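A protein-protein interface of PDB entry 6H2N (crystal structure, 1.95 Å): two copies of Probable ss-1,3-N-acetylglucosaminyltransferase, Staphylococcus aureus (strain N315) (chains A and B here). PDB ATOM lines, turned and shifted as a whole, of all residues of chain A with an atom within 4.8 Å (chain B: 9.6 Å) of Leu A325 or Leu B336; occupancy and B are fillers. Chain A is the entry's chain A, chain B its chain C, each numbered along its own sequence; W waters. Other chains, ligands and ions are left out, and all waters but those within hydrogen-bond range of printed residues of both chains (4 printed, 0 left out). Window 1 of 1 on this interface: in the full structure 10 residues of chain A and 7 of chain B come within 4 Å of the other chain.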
ATOM      1  N   ILE A 322     -24.630  -3.741 -19.111  1.00  0.00           N
ATOM      2  CA  ILE A 322     -23.153  -3.562 -19.074  1.00  0.00           C
ATOM      3  C   ILE A 322     -22.581  -3.831 -17.681  1.00  0.00           C
ATOM      4  O   ILE A 322     -21.393  -4.103 -17.586  1.00  0.00           O
ATOM      5  CB  ILE A 322     -22.691  -2.175 -19.565  1.00  0.00           C
ATOM      6  CG1 ILE A 322     -23.275  -1.039 -18.728  1.00  0.00           C
ATOM      7  CG2 ILE A 322     -22.986  -2.016 -21.042  1.00  0.00           C
ATOM      8  CD1 ILE A 322     -22.549   0.269 -18.901  1.00  0.00           C
ATOM      9  N   PHE A 323     -23.396  -3.711 -16.622  1.00  0.00           N
ATOM     10  CA  PHE A 323     -22.916  -3.899 -15.259  1.00  0.00           C
ATOM     11  C   PHE A 323     -23.095  -5.350 -14.782  1.00  0.00           C
ATOM     12  O   PHE A 323     -22.759  -5.647 -13.651  1.00  0.00           O
ATOM     13  CB  PHE A 323     -23.610  -2.913 -14.309  1.00  0.00           C
ATOM     14  CG  PHE A 323     -23.283  -1.466 -14.576  1.00  0.00           C
ATOM     15  CD1 PHE A 323     -21.978  -1.008 -14.515  1.00  0.00           C
ATOM     16  CD2 PHE A 323     -24.280  -0.563 -14.921  1.00  0.00           C
ATOM     17  CE1 PHE A 323     -21.676   0.326 -14.761  1.00  0.00           C
ATOM     18  CE2 PHE A 323     -23.978   0.773 -15.169  1.00  0.00           C
ATOM     19  CZ  PHE A 323     -22.680   1.220 -15.073  1.00  0.00           C
ATOM     20  N   ASN A 324     -23.572  -6.251 -15.652  1.00  0.00           N
ATOM     21  CA  ASN A 324     -23.890  -7.649 -15.278  1.00  0.00           C
ATOM     22  C   ASN A 324     -22.695  -8.318 -14.582  1.00  0.00           C
ATOM     23  O   ASN A 324     -22.832  -8.923 -13.514  1.00  0.00           O
ATOM     24  CB  ASN A 324     -24.393  -8.463 -16.477  1.00  0.00           C
ATOM     25  CG  ASN A 324     -23.341  -8.833 -17.514  1.00  0.00           C
ATOM     26  OD1 ASN A 324     -22.433  -8.051 -17.843  1.00  0.00           O
ATOM     27  ND2 ASN A 324     -23.470 -10.036 -18.054  1.00  0.00           N
ATOM     28  N   LEU A 325     -21.508  -8.178 -15.169  1.00  0.00           N
ATOM     29  CA  LEU A 325     -20.325  -8.856 -14.654  1.00  0.00           C
ATOM     30  C   LEU A 325     -19.885  -8.194 -13.344  1.00  0.00           C
ATOM     31  O   LEU A 325     -19.622  -8.871 -12.342  1.00  0.00           O
ATOM     32  CB  LEU A 325     -19.217  -8.847 -15.709  1.00  0.00           C
ATOM     33  CG  LEU A 325     -17.834  -9.281 -15.217  1.00  0.00           C
ATOM     34  CD1 LEU A 325     -17.831 -10.738 -14.769  1.00  0.00           C
ATOM     35  CD2 LEU A 325     -16.793  -9.042 -16.302  1.00  0.00           C
ATOM     36  N   LYS A 326     -19.810  -6.862 -13.342  1.00  0.00           N
ATOM     37  CA  LYS A 326     -19.381  -6.177 -12.148  1.00  0.00           C
ATOM     38  C   LYS A 326     -20.299  -6.576 -10.993  1.00  0.00           C
ATOM     39  O   LYS A 326     -19.848  -6.841  -9.907  1.00  0.00           O
ATOM     40  CB  LYS A 326     -19.360  -4.653 -12.321  1.00  0.00           C
ATOM     41  CG  LYS A 326     -18.790  -3.908 -11.122  1.00  0.00           C
ATOM     42  CD  LYS A 326     -18.225  -2.576 -11.495  1.00  0.00           C
ATOM     43  CE  LYS A 326     -17.657  -1.823 -10.317  1.00  0.00           C
ATOM     44  NZ  LYS A 326     -17.216  -0.479 -10.745  1.00  0.00           N
ATOM     45  N   LEU A 327     -21.605  -6.597 -11.261  1.00  0.00           N
ATOM     46  CA  LEU A 327     -22.585  -6.825 -10.194  1.00  0.00           C
ATOM     47  C   LEU A 327     -22.377  -8.240  -9.639  1.00  0.00           C
ATOM     48  O   LEU A 327     -22.341  -8.415  -8.456  1.00  0.00           O
ATOM     49  CB  LEU A 327     -24.003  -6.635 -10.744  1.00  0.00           C
ATOM     50  CG  LEU A 327     -25.120  -6.882  -9.738  1.00  0.00           C
ATOM     51  CD1 LEU A 327     -24.895  -6.053  -8.486  1.00  0.00           C
ATOM     52  CD2 LEU A 327     -26.476  -6.581 -10.362  1.00  0.00           C
ATOM     53  N   GLU A 328     -22.190  -9.226 -10.522  1.00  0.00           N
ATOM     54  CA  GLU A 328     -21.991 -10.625 -10.090  1.00  0.00           C
ATOM     55  C   GLU A 328     -20.664 -10.744  -9.322  1.00  0.00           C
ATOM     56  O   GLU A 328     -20.596 -11.426  -8.290  1.00  0.00           O
ATOM     57  CB  GLU A 328     -22.061 -11.582 -11.282  1.00  0.00           C
ATOM     58  CG  GLU A 328     -22.180 -13.057 -10.888  1.00  0.00           C
ATOM     59  CD  GLU A 328     -23.388 -13.334  -9.994  1.00  0.00           C
ATOM     60  OE1 GLU A 328     -24.512 -12.891 -10.382  1.00  0.00           O
ATOM     61  OE2 GLU A 328     -23.207 -13.935  -8.883  1.00  0.00           O
ATOM     62  N   ALA A 329     -19.618 -10.064  -9.815  1.00  0.00           N
ATOM     63  CA  ALA A 329     -18.306 -10.022  -9.147  1.00  0.00           C
ATOM     64  C   ALA A 329     -18.482  -9.570  -7.696  1.00  0.00           C
ATOM     65  O   ALA A 329     -17.929 -10.183  -6.783  1.00  0.00           O
ATOM     66  CB  ALA A 329     -17.354  -9.109  -9.894  1.00  0.00           C
ATOM     67  N   GLN A 332     -20.269 -12.172  -5.639  1.00  0.00           N
ATOM     68  CA  GLN A 332     -19.357 -13.267  -5.375  1.00  0.00           C
ATOM     69  C   GLN A 332     -18.188 -12.847  -4.461  1.00  0.00           C
ATOM     70  O   GLN A 332     -17.354 -13.683  -4.135  1.00  0.00           O
ATOM     71  CB  GLN A 332     -18.785 -13.811  -6.680  1.00  0.00           C
ATOM     72  CG  GLN A 332     -19.818 -14.381  -7.637  1.00  0.00           C
ATOM     73  CD  GLN A 332     -20.516 -15.616  -7.118  1.00  0.00           C
ATOM     74  OE1 GLN A 332     -19.961 -16.373  -6.331  1.00  0.00           O
ATOM     75  NE2 GLN A 332     -21.753 -15.820  -7.555  1.00  0.00           N
ATOM     76  N   ASP A 334     -15.449 -11.143  -5.137  1.00  0.00           N
ATOM     77  CA  ASP A 334     -14.251 -11.546  -5.913  1.00  0.00           C
ATOM     78  C   ASP A 334     -13.565 -10.285  -6.466  1.00  0.00           C
ATOM     79  O   ASP A 334     -13.995  -9.742  -7.460  1.00  0.00           O
ATOM     80  CB  ASP A 334     -14.686 -12.524  -7.001  1.00  0.00           C
ATOM     81  CG  ASP A 334     -13.579 -13.153  -7.830  1.00  0.00           C
ATOM     82  OD1 ASP A 334     -12.597 -12.475  -8.143  1.00  0.00           O
ATOM     83  OD2 ASP A 334     -13.761 -14.289  -8.207  1.00  0.00           O
ATOM     84  N   ALA A 337     -12.295 -10.307 -10.013  1.00  0.00           N
ATOM     85  CA  ALA A 337     -13.361 -10.179 -10.983  1.00  0.00           C
ATOM     86  C   ALA A 337     -13.836  -8.722 -11.074  1.00  0.00           C
ATOM     87  O   ALA A 337     -14.190  -8.269 -12.169  1.00  0.00           O
ATOM     88  CB  ALA A 337     -14.492 -11.128 -10.676  1.00  0.00           C
ATOM     89  N   ALA A 341     -13.747  -6.531 -14.377  1.00  0.00           N
ATOM     90  CA  ALA A 341     -14.987  -5.906 -14.801  1.00  0.00           C
ATOM     91  C   ALA A 341     -14.747  -4.425 -15.128  1.00  0.00           C
ATOM     92  O   ALA A 341     -15.201  -3.911 -16.154  1.00  0.00           O
ATOM     93  CB  ALA A 341     -16.049  -6.071 -13.731  1.00  0.00           C
ATOM     94  N   LEU A 344     -13.030  -3.768 -18.363  1.00  0.00           N
ATOM     95  CA  LEU A 344     -13.843  -4.010 -19.563  1.00  0.00           C
ATOM     96  C   LEU A 344     -14.936  -2.951 -19.733  1.00  0.00           C
ATOM     97  O   LEU A 344     -15.533  -2.866 -20.794  1.00  0.00           O
ATOM     98  CB  LEU A 344     -14.446  -5.417 -19.494  1.00  0.00           C
ATOM     99  CG  LEU A 344     -13.412  -6.538 -19.436  1.00  0.00           C
ATOM    100  CD1 LEU A 344     -14.079  -7.894 -19.297  1.00  0.00           C
ATOM    101  CD2 LEU A 344     -12.532  -6.499 -20.668  1.00  0.00           C
ATOM    102  N   PHE B 287     -24.508 -18.856 -22.816  1.00  0.00           N
ATOM    103  CA  PHE B 287     -25.386 -18.829 -21.652  1.00  0.00           C
ATOM    104  C   PHE B 287     -24.877 -17.844 -20.580  1.00  0.00           C
ATOM    105  O   PHE B 287     -25.695 -17.266 -19.829  1.00  0.00           O
ATOM    106  CB  PHE B 287     -25.532 -20.230 -21.054  1.00  0.00           C
ATOM    107  CG  PHE B 287     -24.364 -20.674 -20.222  1.00  0.00           C
ATOM    108  CD1 PHE B 287     -23.250 -21.244 -20.813  1.00  0.00           C
ATOM    109  CD2 PHE B 287     -24.366 -20.484 -18.845  1.00  0.00           C
ATOM    110  CE1 PHE B 287     -22.155 -21.615 -20.052  1.00  0.00           C
ATOM    111  CE2 PHE B 287     -23.265 -20.853 -18.085  1.00  0.00           C
ATOM    112  CZ  PHE B 287     -22.159 -21.408 -18.691  1.00  0.00           C
ATOM    113  N   ALA B 288     -23.551 -17.655 -20.483  1.00  0.00           N
ATOM    114  CA  ALA B 288     -22.955 -17.026 -19.280  1.00  0.00           C
ATOM    115  C   ALA B 288     -23.432 -15.575 -19.089  1.00  0.00           C
ATOM    116  O   ALA B 288     -23.670 -15.166 -17.948  1.00  0.00           O
ATOM    117  CB  ALA B 288     -21.447 -17.099 -19.315  1.00  0.00           C
ATOM    118  N   ASN B 289     -23.541 -14.799 -20.171  1.00  0.00           N
ATOM    119  CA  ASN B 289     -23.912 -13.369 -20.067  1.00  0.00           C
ATOM    120  C   ASN B 289     -25.397 -13.152 -20.412  1.00  0.00           C
ATOM    121  O   ASN B 289     -25.809 -12.023 -20.649  1.00  0.00           O
ATOM    122  CB  ASN B 289     -23.014 -12.515 -20.962  1.00  0.00           C
ATOM    123  CG  ASN B 289     -21.616 -12.373 -20.409  1.00  0.00           C
ATOM    124  OD1 ASN B 289     -21.417 -11.767 -19.349  1.00  0.00           O
ATOM    125  ND2 ASN B 289     -20.642 -12.902 -21.123  1.00  0.00           N
ATOM    126  N   SER B 290     -26.168 -14.249 -20.467  1.00  0.00           N
ATOM    127  CA  SER B 290     -27.549 -14.285 -20.956  1.00  0.00           C
ATOM    128  C   SER B 290     -28.506 -13.823 -19.852  1.00  0.00           C
ATOM    129  O   SER B 290     -28.091 -13.625 -18.716  1.00  0.00           O
ATOM    130  CB  SER B 290     -27.911 -15.682 -21.424  1.00  0.00           C
ATOM    131  OG  SER B 290     -28.130 -16.555 -20.323  1.00  0.00           O
ATOM    132  N   TYR B 294     -29.563 -16.851 -12.544  1.00  0.00           N
ATOM    133  CA  TYR B 294     -28.268 -17.188 -11.988  1.00  0.00           C
ATOM    134  C   TYR B 294     -28.193 -18.669 -11.601  1.00  0.00           C
ATOM    135  O   TYR B 294     -27.237 -19.356 -11.955  1.00  0.00           O
ATOM    136  CB  TYR B 294     -27.961 -16.338 -10.757  1.00  0.00           C
ATOM    137  CG  TYR B 294     -26.744 -16.786 -10.001  1.00  0.00           C
ATOM    138  CD1 TYR B 294     -25.464 -16.509 -10.467  1.00  0.00           C
ATOM    139  CD2 TYR B 294     -26.869 -17.517  -8.832  1.00  0.00           C
ATOM    140  CE1 TYR B 294     -24.334 -16.939  -9.784  1.00  0.00           C
ATOM    141  CE2 TYR B 294     -25.750 -17.940  -8.131  1.00  0.00           C
ATOM    142  CZ  TYR B 294     -24.484 -17.660  -8.613  1.00  0.00           C
ATOM    143  OH  TYR B 294     -23.405 -18.089  -7.906  1.00  0.00           O
ATOM    144  N   LYS B 297     -27.846 -20.844 -14.589  1.00  0.00           N
ATOM    145  CA  LYS B 297     -26.505 -20.724 -15.133  1.00  0.00           C
ATOM    146  C   LYS B 297     -25.552 -21.652 -14.374  1.00  0.00           C
ATOM    147  O   LYS B 297     -24.707 -22.324 -15.010  1.00  0.00           O
ATOM    148  CB  LYS B 297     -25.974 -19.294 -15.071  1.00  0.00           C
ATOM    149  CG  LYS B 297     -26.628 -18.337 -16.049  1.00  0.00           C
ATOM    150  CD  LYS B 297     -26.237 -16.900 -15.830  1.00  0.00           C
ATOM    151  CE  LYS B 297     -26.727 -16.004 -16.943  1.00  0.00           C
ATOM    152  NZ  LYS B 297     -26.151 -14.647 -16.815  1.00  0.00           N
ATOM    153  N   ILE B 298     -25.673 -21.662 -13.036  1.00  0.00           N
ATOM    154  CA  ILE B 298     -24.784 -22.454 -12.204  1.00  0.00           C
ATOM    155  C   ILE B 298     -25.021 -23.940 -12.518  1.00  0.00           C
ATOM    156  O   ILE B 298     -24.060 -24.698 -12.663  1.00  0.00           O
ATOM    157  CB  ILE B 298     -24.915 -22.112 -10.703  1.00  0.00           C
ATOM    158  CG1 ILE B 298     -24.322 -20.734 -10.384  1.00  0.00           C
ATOM    159  CG2 ILE B 298     -24.282 -23.176  -9.815  1.00  0.00           C
ATOM    160  CD1 ILE B 298     -22.814 -20.655 -10.516  1.00  0.00           C
ATOM    161  N   LEU B 301     -23.634 -24.817 -16.102  1.00  0.00           N
ATOM    162  CA  LEU B 301     -22.201 -24.838 -16.145  1.00  0.00           C
ATOM    163  C   LEU B 301     -21.657 -26.032 -15.359  1.00  0.00           C
ATOM    164  O   LEU B 301     -20.660 -26.596 -15.757  1.00  0.00           O
ATOM    165  CB  LEU B 301     -21.621 -23.530 -15.600  1.00  0.00           C
ATOM    166  CG  LEU B 301     -20.096 -23.484 -15.468  1.00  0.00           C
ATOM    167  CD1 LEU B 301     -19.417 -23.766 -16.797  1.00  0.00           C
ATOM    168  CD2 LEU B 301     -19.657 -22.135 -14.907  1.00  0.00           C
ATOM    169  N   LEU B 325      -9.237 -19.698 -23.042  1.00  0.00           N
ATOM    170  CA  LEU B 325      -9.692 -19.196 -21.736  1.00  0.00           C
ATOM    171  C   LEU B 325     -11.099 -19.721 -21.416  1.00  0.00           C
ATOM    172  O   LEU B 325     -11.350 -20.160 -20.298  1.00  0.00           O
ATOM    173  CB  LEU B 325      -9.675 -17.664 -21.713  1.00  0.00           C
ATOM    174  CG  LEU B 325     -10.375 -17.040 -20.505  1.00  0.00           C
ATOM    175  CD1 LEU B 325      -9.635 -17.377 -19.217  1.00  0.00           C
ATOM    176  CD2 LEU B 325     -10.504 -15.531 -20.683  1.00  0.00           C
ATOM    177  N   LYS B 326     -12.006 -19.675 -22.397  1.00  0.00           N
ATOM    178  CA  LYS B 326     -13.373 -20.131 -22.177  1.00  0.00           C
ATOM    179  C   LYS B 326     -13.370 -21.606 -21.752  1.00  0.00           C
ATOM    180  O   LYS B 326     -14.109 -22.006 -20.813  1.00  0.00           O
ATOM    181  CB  LYS B 326     -14.248 -19.917 -23.415  1.00  0.00           C
ATOM    182  CG  LYS B 326     -15.700 -20.296 -23.195  1.00  0.00           C
ATOM    183  CD  LYS B 326     -16.613 -19.891 -24.317  1.00  0.00           C
ATOM    184  CE  LYS B 326     -18.078 -19.988 -23.932  1.00  0.00           C
ATOM    185  NZ  LYS B 326     -18.935 -19.314 -24.931  1.00  0.00           N
ATOM    186  N   ALA B 329     -12.058 -22.004 -18.218  1.00  0.00           N
ATOM    187  CA  ALA B 329     -13.072 -21.484 -17.285  1.00  0.00           C
ATOM    188  C   ALA B 329     -14.179 -22.522 -17.055  1.00  0.00           C
ATOM    189  O   ALA B 329     -14.605 -22.718 -15.907  1.00  0.00           O
ATOM    190  CB  ALA B 329     -13.617 -20.190 -17.817  1.00  0.00           C
ATOM    191  N   ILE B 330     -14.609 -23.210 -18.122  1.00  0.00           N
ATOM    192  CA  ILE B 330     -15.585 -24.323 -18.011  1.00  0.00           C
ATOM    193  C   ILE B 330     -14.973 -25.474 -17.211  1.00  0.00           C
ATOM    194  O   ILE B 330     -15.618 -26.008 -16.314  1.00  0.00           O
ATOM    195  CB  ILE B 330     -16.092 -24.782 -19.392  1.00  0.00           C
ATOM    196  CG1 ILE B 330     -16.922 -23.688 -20.061  1.00  0.00           C
ATOM    197  CG2 ILE B 330     -16.859 -26.105 -19.299  1.00  0.00           C
ATOM    198  CD1 ILE B 330     -16.878 -23.718 -21.567  1.00  0.00           C
ATOM    199  N   GLN B 332     -12.881 -25.253 -14.918  1.00  0.00           N
ATOM    200  CA  GLN B 332     -12.741 -24.771 -13.549  1.00  0.00           C
ATOM    201  C   GLN B 332     -14.126 -24.524 -12.919  1.00  0.00           C
ATOM    202  O   GLN B 332     -14.231 -24.279 -11.722  1.00  0.00           O
ATOM    203  CB  GLN B 332     -11.927 -23.472 -13.517  1.00  0.00           C
ATOM    204  CG  GLN B 332     -10.467 -23.579 -13.945  1.00  0.00           C
ATOM    205  CD  GLN B 332      -9.642 -24.473 -13.066  1.00  0.00           C
ATOM    206  OE1 GLN B 332      -9.924 -24.616 -11.898  1.00  0.00           O
ATOM    207  NE2 GLN B 332      -8.614 -25.092 -13.629  1.00  0.00           N
ATOM    208  N   ASN B 333     -15.188 -24.551 -13.733  1.00  0.00           N
ATOM    209  CA  ASN B 333     -16.560 -24.445 -13.237  1.00  0.00           C
ATOM    210  C   ASN B 333     -16.700 -23.069 -12.568  1.00  0.00           C
ATOM    211  O   ASN B 333     -17.194 -22.945 -11.468  1.00  0.00           O
ATOM    212  CB  ASN B 333     -16.897 -25.627 -12.315  1.00  0.00           C
ATOM    213  CG  ASN B 333     -18.375 -25.794 -12.030  1.00  0.00           C
ATOM    214  OD1 ASN B 333     -19.227 -25.412 -12.826  1.00  0.00           O
ATOM    215  ND2 ASN B 333     -18.691 -26.375 -10.887  1.00  0.00           N
ATOM    216  N   ASP B 334     -16.246 -22.039 -13.284  1.00  0.00           N
ATOM    217  CA  ASP B 334     -16.133 -20.692 -12.798  1.00  0.00           C
ATOM    218  C   ASP B 334     -16.969 -19.747 -13.674  1.00  0.00           C
ATOM    219  O   ASP B 334     -16.534 -19.335 -14.757  1.00  0.00           O
ATOM    220  CB  ASP B 334     -14.665 -20.293 -12.792  1.00  0.00           C
ATOM    221  CG  ASP B 334     -14.409 -18.935 -12.158  1.00  0.00           C
ATOM    222  OD1 ASP B 334     -15.141 -17.974 -12.450  1.00  0.00           O
ATOM    223  OD2 ASP B 334     -13.449 -18.857 -11.409  1.00  0.00           O
ATOM    224  N   LEU B 335     -18.186 -19.418 -13.217  1.00  0.00           N
ATOM    225  CA  LEU B 335     -19.120 -18.664 -14.053  1.00  0.00           C
ATOM    226  C   LEU B 335     -18.522 -17.293 -14.399  1.00  0.00           C
ATOM    227  O   LEU B 335     -18.616 -16.863 -15.516  1.00  0.00           O
ATOM    228  CB  LEU B 335     -20.474 -18.550 -13.348  1.00  0.00           C
ATOM    229  CG  LEU B 335     -21.542 -17.763 -14.108  1.00  0.00           C
ATOM    230  CD1 LEU B 335     -21.946 -18.470 -15.394  1.00  0.00           C
ATOM    231  CD2 LEU B 335     -22.762 -17.514 -13.228  1.00  0.00           C
ATOM    232  N   LEU B 336     -17.863 -16.636 -13.439  1.00  0.00           N
ATOM    233  CA  LEU B 336     -17.306 -15.277 -13.676  1.00  0.00           C
ATOM    234  C   LEU B 336     -16.288 -15.350 -14.816  1.00  0.00           C
ATOM    235  O   LEU B 336     -16.286 -14.516 -15.684  1.00  0.00           O
ATOM    236  CB  LEU B 336     -16.680 -14.718 -12.396  1.00  0.00           C
ATOM    237  CG  LEU B 336     -17.651 -14.173 -11.346  1.00  0.00           C
ATOM    238  CD1 LEU B 336     -16.911 -13.860 -10.060  1.00  0.00           C
ATOM    239  CD2 LEU B 336     -18.392 -12.927 -11.830  1.00  0.00           C
ATOM    240  N   ALA B 337     -15.450 -16.386 -14.800  1.00  0.00           N
ATOM    241  CA  ALA B 337     -14.402 -16.598 -15.822  1.00  0.00           C
ATOM    242  C   ALA B 337     -15.029 -16.861 -17.200  1.00  0.00           C
ATOM    243  O   ALA B 337     -14.552 -16.341 -18.200  1.00  0.00           O
ATOM    244  CB  ALA B 337     -13.487 -17.711 -15.404  1.00  0.00           C
ATOM    245  N   VAL B 338     -16.144 -17.591 -17.243  1.00  0.00           N
ATOM    246  CA  VAL B 338     -16.847 -17.825 -18.521  1.00  0.00           C
ATOM    247  C   VAL B 338     -17.446 -16.511 -19.019  1.00  0.00           C
ATOM    248  O   VAL B 338     -17.324 -16.181 -20.187  1.00  0.00           O
ATOM    249  CB  VAL B 338     -17.915 -18.933 -18.437  1.00  0.00           C
ATOM    250  CG1 VAL B 338     -18.601 -19.155 -19.781  1.00  0.00           C
ATOM    251  CG2 VAL B 338     -17.351 -20.241 -17.899  1.00  0.00           C
ATOM    252  N   MET B 339     -18.106 -15.762 -18.124  1.00  0.00           N
ATOM    253  CA  MET B 339     -18.633 -14.446 -18.467  1.00  0.00           C
ATOM    254  C   MET B 339     -17.527 -13.572 -19.079  1.00  0.00           C
ATOM    255  O   MET B 339     -17.735 -12.934 -20.113  1.00  0.00           O
ATOM    256  CB  MET B 339     -19.209 -13.737 -17.235  1.00  0.00           C
ATOM    257  CG  MET B 339     -20.521 -14.329 -16.792  1.00  0.00           C
ATOM    258  SD  MET B 339     -21.077 -13.660 -15.230  1.00  0.00           S
ATOM    259  CE  MET B 339     -21.665 -12.044 -15.734  1.00  0.00           C
ATOM    260  N   ILE B 340     -16.363 -13.548 -18.434  1.00  0.00           N
ATOM    261  CA  ILE B 340     -15.249 -12.745 -18.904  1.00  0.00           C
ATOM    262  C   ILE B 340     -14.774 -13.250 -20.282  1.00  0.00           C
ATOM    263  O   ILE B 340     -14.532 -12.464 -21.192  1.00  0.00           O
ATOM    264  CB  ILE B 340     -14.125 -12.733 -17.852  1.00  0.00           C
ATOM    265  CG1 ILE B 340     -14.582 -12.008 -16.581  1.00  0.00           C
ATOM    266  CG2 ILE B 340     -12.853 -12.116 -18.411  1.00  0.00           C
ATOM    267  CD1 ILE B 340     -13.727 -12.301 -15.367  1.00  0.00           C
ATOM    268  N   ALA B 341     -14.627 -14.562 -20.419  1.00  0.00           N
ATOM    269  CA  ALA B 341     -14.131 -15.148 -21.689  1.00  0.00           C
ATOM    270  C   ALA B 341     -15.042 -14.702 -22.843  1.00  0.00           C
ATOM    271  O   ALA B 341     -14.565 -14.303 -23.887  1.00  0.00           O
ATOM    272  CB  ALA B 341     -14.069 -16.642 -21.571  1.00  0.00           C
ATOM    273  N   ASP B 342     -16.363 -14.689 -22.611  1.00  0.00           N
ATOM    274  CA  ASP B 342     -17.332 -14.348 -23.659  1.00  0.00           C
ATOM    275  C   ASP B 342     -17.248 -12.860 -24.008  1.00  0.00           C
ATOM    276  O   ASP B 342     -17.435 -12.533 -25.155  1.00  0.00           O
ATOM    277  CB  ASP B 342     -18.764 -14.752 -23.292  1.00  0.00           C
ATOM    278  CG  ASP B 342     -19.048 -16.219 -23.525  1.00  0.00           C
ATOM    279  OD1 ASP B 342     -18.225 -16.866 -24.210  1.00  0.00           O
ATOM    280  OD2 ASP B 342     -20.054 -16.723 -22.986  1.00  0.00           O
ATOM    281  N   LYS B 343     -16.963 -11.984 -23.029  1.00  0.00           N
ATOM    282  CA  LYS B 343     -16.800 -10.551 -23.289  1.00  0.00           C
ATOM    283  C   LYS B 343     -15.560 -10.288 -24.159  1.00  0.00           C
ATOM    284  O   LYS B 343     -15.515  -9.286 -24.885  1.00  0.00           O
ATOM    285  CB  LYS B 343     -16.739  -9.763 -21.972  1.00  0.00           C
ATOM    286  CG  LYS B 343     -18.109  -9.507 -21.347  1.00  0.00           C
ATOM    287  CD  LYS B 343     -18.031  -8.939 -19.953  1.00  0.00           C
ATOM    288  CE  LYS B 343     -19.377  -8.775 -19.268  1.00  0.00           C
ATOM    289  NZ  LYS B 343     -20.434  -8.238 -20.161  1.00  0.00           N
ATOM    290  N   LEU B 344     -14.540 -11.142 -24.032  1.00  0.00           N
ATOM    291  CA  LEU B 344     -13.285 -10.979 -24.767  1.00  0.00           C
ATOM    292  C   LEU B 344     -13.351 -11.625 -26.164  1.00  0.00           C
ATOM    293  O   LEU B 344     -12.607 -11.229 -27.041  1.00  0.00           O
ATOM    294  CB  LEU B 344     -12.146 -11.544 -23.915  1.00  0.00           C
ATOM    295  CG  LEU B 344     -11.904 -10.757 -22.627  1.00  0.00           C
ATOM    296  CD1 LEU B 344     -10.958 -11.488 -21.703  1.00  0.00           C
ATOM    297  CD2 LEU B 344     -11.404  -9.351 -22.923  1.00  0.00           C
HETATM  298  O   HOH W   1     -15.342 -17.165  -9.149  1.00  0.00           O
HETATM  299  O   HOH W   2     -25.334 -11.768 -16.737  1.00  0.00           O
HETATM  300  O   HOH W   3     -19.305  -5.177 -19.291  1.00  0.00           O
HETATM  301  O   HOH W   4     -23.180  -6.923 -20.915  1.00  0.00           O
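Of chain B, only Leu B336, Met B339, Ile B340 and Lys B343 come within 4 Å of Leu A325. Leu B336 touches just these residues of chain A: Leu A325 (3.7 Å), Glu A328 (3.9 Å), Ala A329 (3.7 Å), Gln A332 (3.8 Å), Asp A334 (3.7 Å) and Ala A337 (3.7 Å). Asn A324 touches three residues of chain B. Ala A329 touches just one residue of chain B: Leu B336. Of the printed residues of chain A, Tyr B294 touches Glu A328 (3.3 Å) and Gln A332 (2.8 Å). Of the printed residues of chain A, Leu B344 touches Leu A344. Printed residues of chain B within 4 Å of Glu A328: Tyr B294 and Leu B336. The nearest residue of chain B that does not touch Leu A325 is Asn B289 (5.2 Å). The nearest printed residue of chain A that does not touch Leu B336 is Asn A324 (6.2 Å). The nearest printed residue of chain A that does not touch Leu B344 is Leu A325 (8.2 Å).
Water W2 bridges ND2 of Asn A324 (2.9 Å) and NZ of Lys B297 (3.0 Å). Water W3 lies within hydrogen-bond range of the backbone carbonyl oxygen of Ile A322 (2.9 Å) and the side-chain amino group of Lys B343 (3.4 Å). Water W4 lies within hydrogen-bond range of the side-chain amino group of Lys B343 (3.1 Å) and the side-chain amide oxygen of Asn A324 (3.4 Å). Water W1 lies within hydrogen-bond range of the side-chain carboxylate of Asp B334 (3.4 Å) and the side-chain carboxylate of Asp A334 (3.4 Å).
Leu A344 touches its own counterpart, Leu B344. Positions printed for both chains: 325, 326, 329, 332, 334, 337, 341 and 344.
The side-chain carboxylate (OE2) of Glu A328 lies within hydrogen-bond range of the side-chain amide nitrogen (NE2) of Gln A332 (2.7 Å). O of Ala A329 lies within hydrogen-bond range of N of Asp A334 (3.1 Å). The side-chain carboxylate (OD1) of Asp A334 lies within hydrogen-bond range of the backbone NH (N) of Ala A337. The side-chain amide nitrogen of Asn B289 is in hydrogen-bond range of the backbone carbonyl oxygen of Met B339 (3.1 Å). OD1 of Asp B334 sits at hydrogen-bond distance from N of Leu B336 (3.2 Å).
ND2 of Asn A324 sits at hydrogen-bond distance from OD1 of Asn B289, at 3.0 Å. OD1 of Asn A324 sits at hydrogen-bond distance from NZ of Lys B343 (3.1 Å). The side-chain amide nitrogen (NE2) of Gln A332 lies within hydrogen-bond range of the side-chain hydroxyl (OH) of Tyr B294 (2.8 Å).
Printed residues of chain B that touch a printed residue of chain A: Asn B289, Tyr B294, Leu B336, Met B339, Ile B340, Lys B343 and Leu B344. Hydrophobic or aromatic side chains of chain B that line the printed part of chain A: Tyr B294, Leu B336, Met B339, Ile B340 and Leu B344. Among the printed residues, 15 pairs touch across the chains.
Among the printed residues, merely in contact across the chains: Glu A328 with Tyr B294, Asn A324 with Met B339, Leu A325 with Lys B343, Leu A325 with Met B339, Asp A334 with Leu B336, Ala A337 with Leu B336, Leu A325 with Leu B336, Ala A329 with Leu B336, Leu A325 with Ile B340, Leu A344 with Leu B344, Gln A332 with Leu B336 and Glu A328 with Leu B336.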
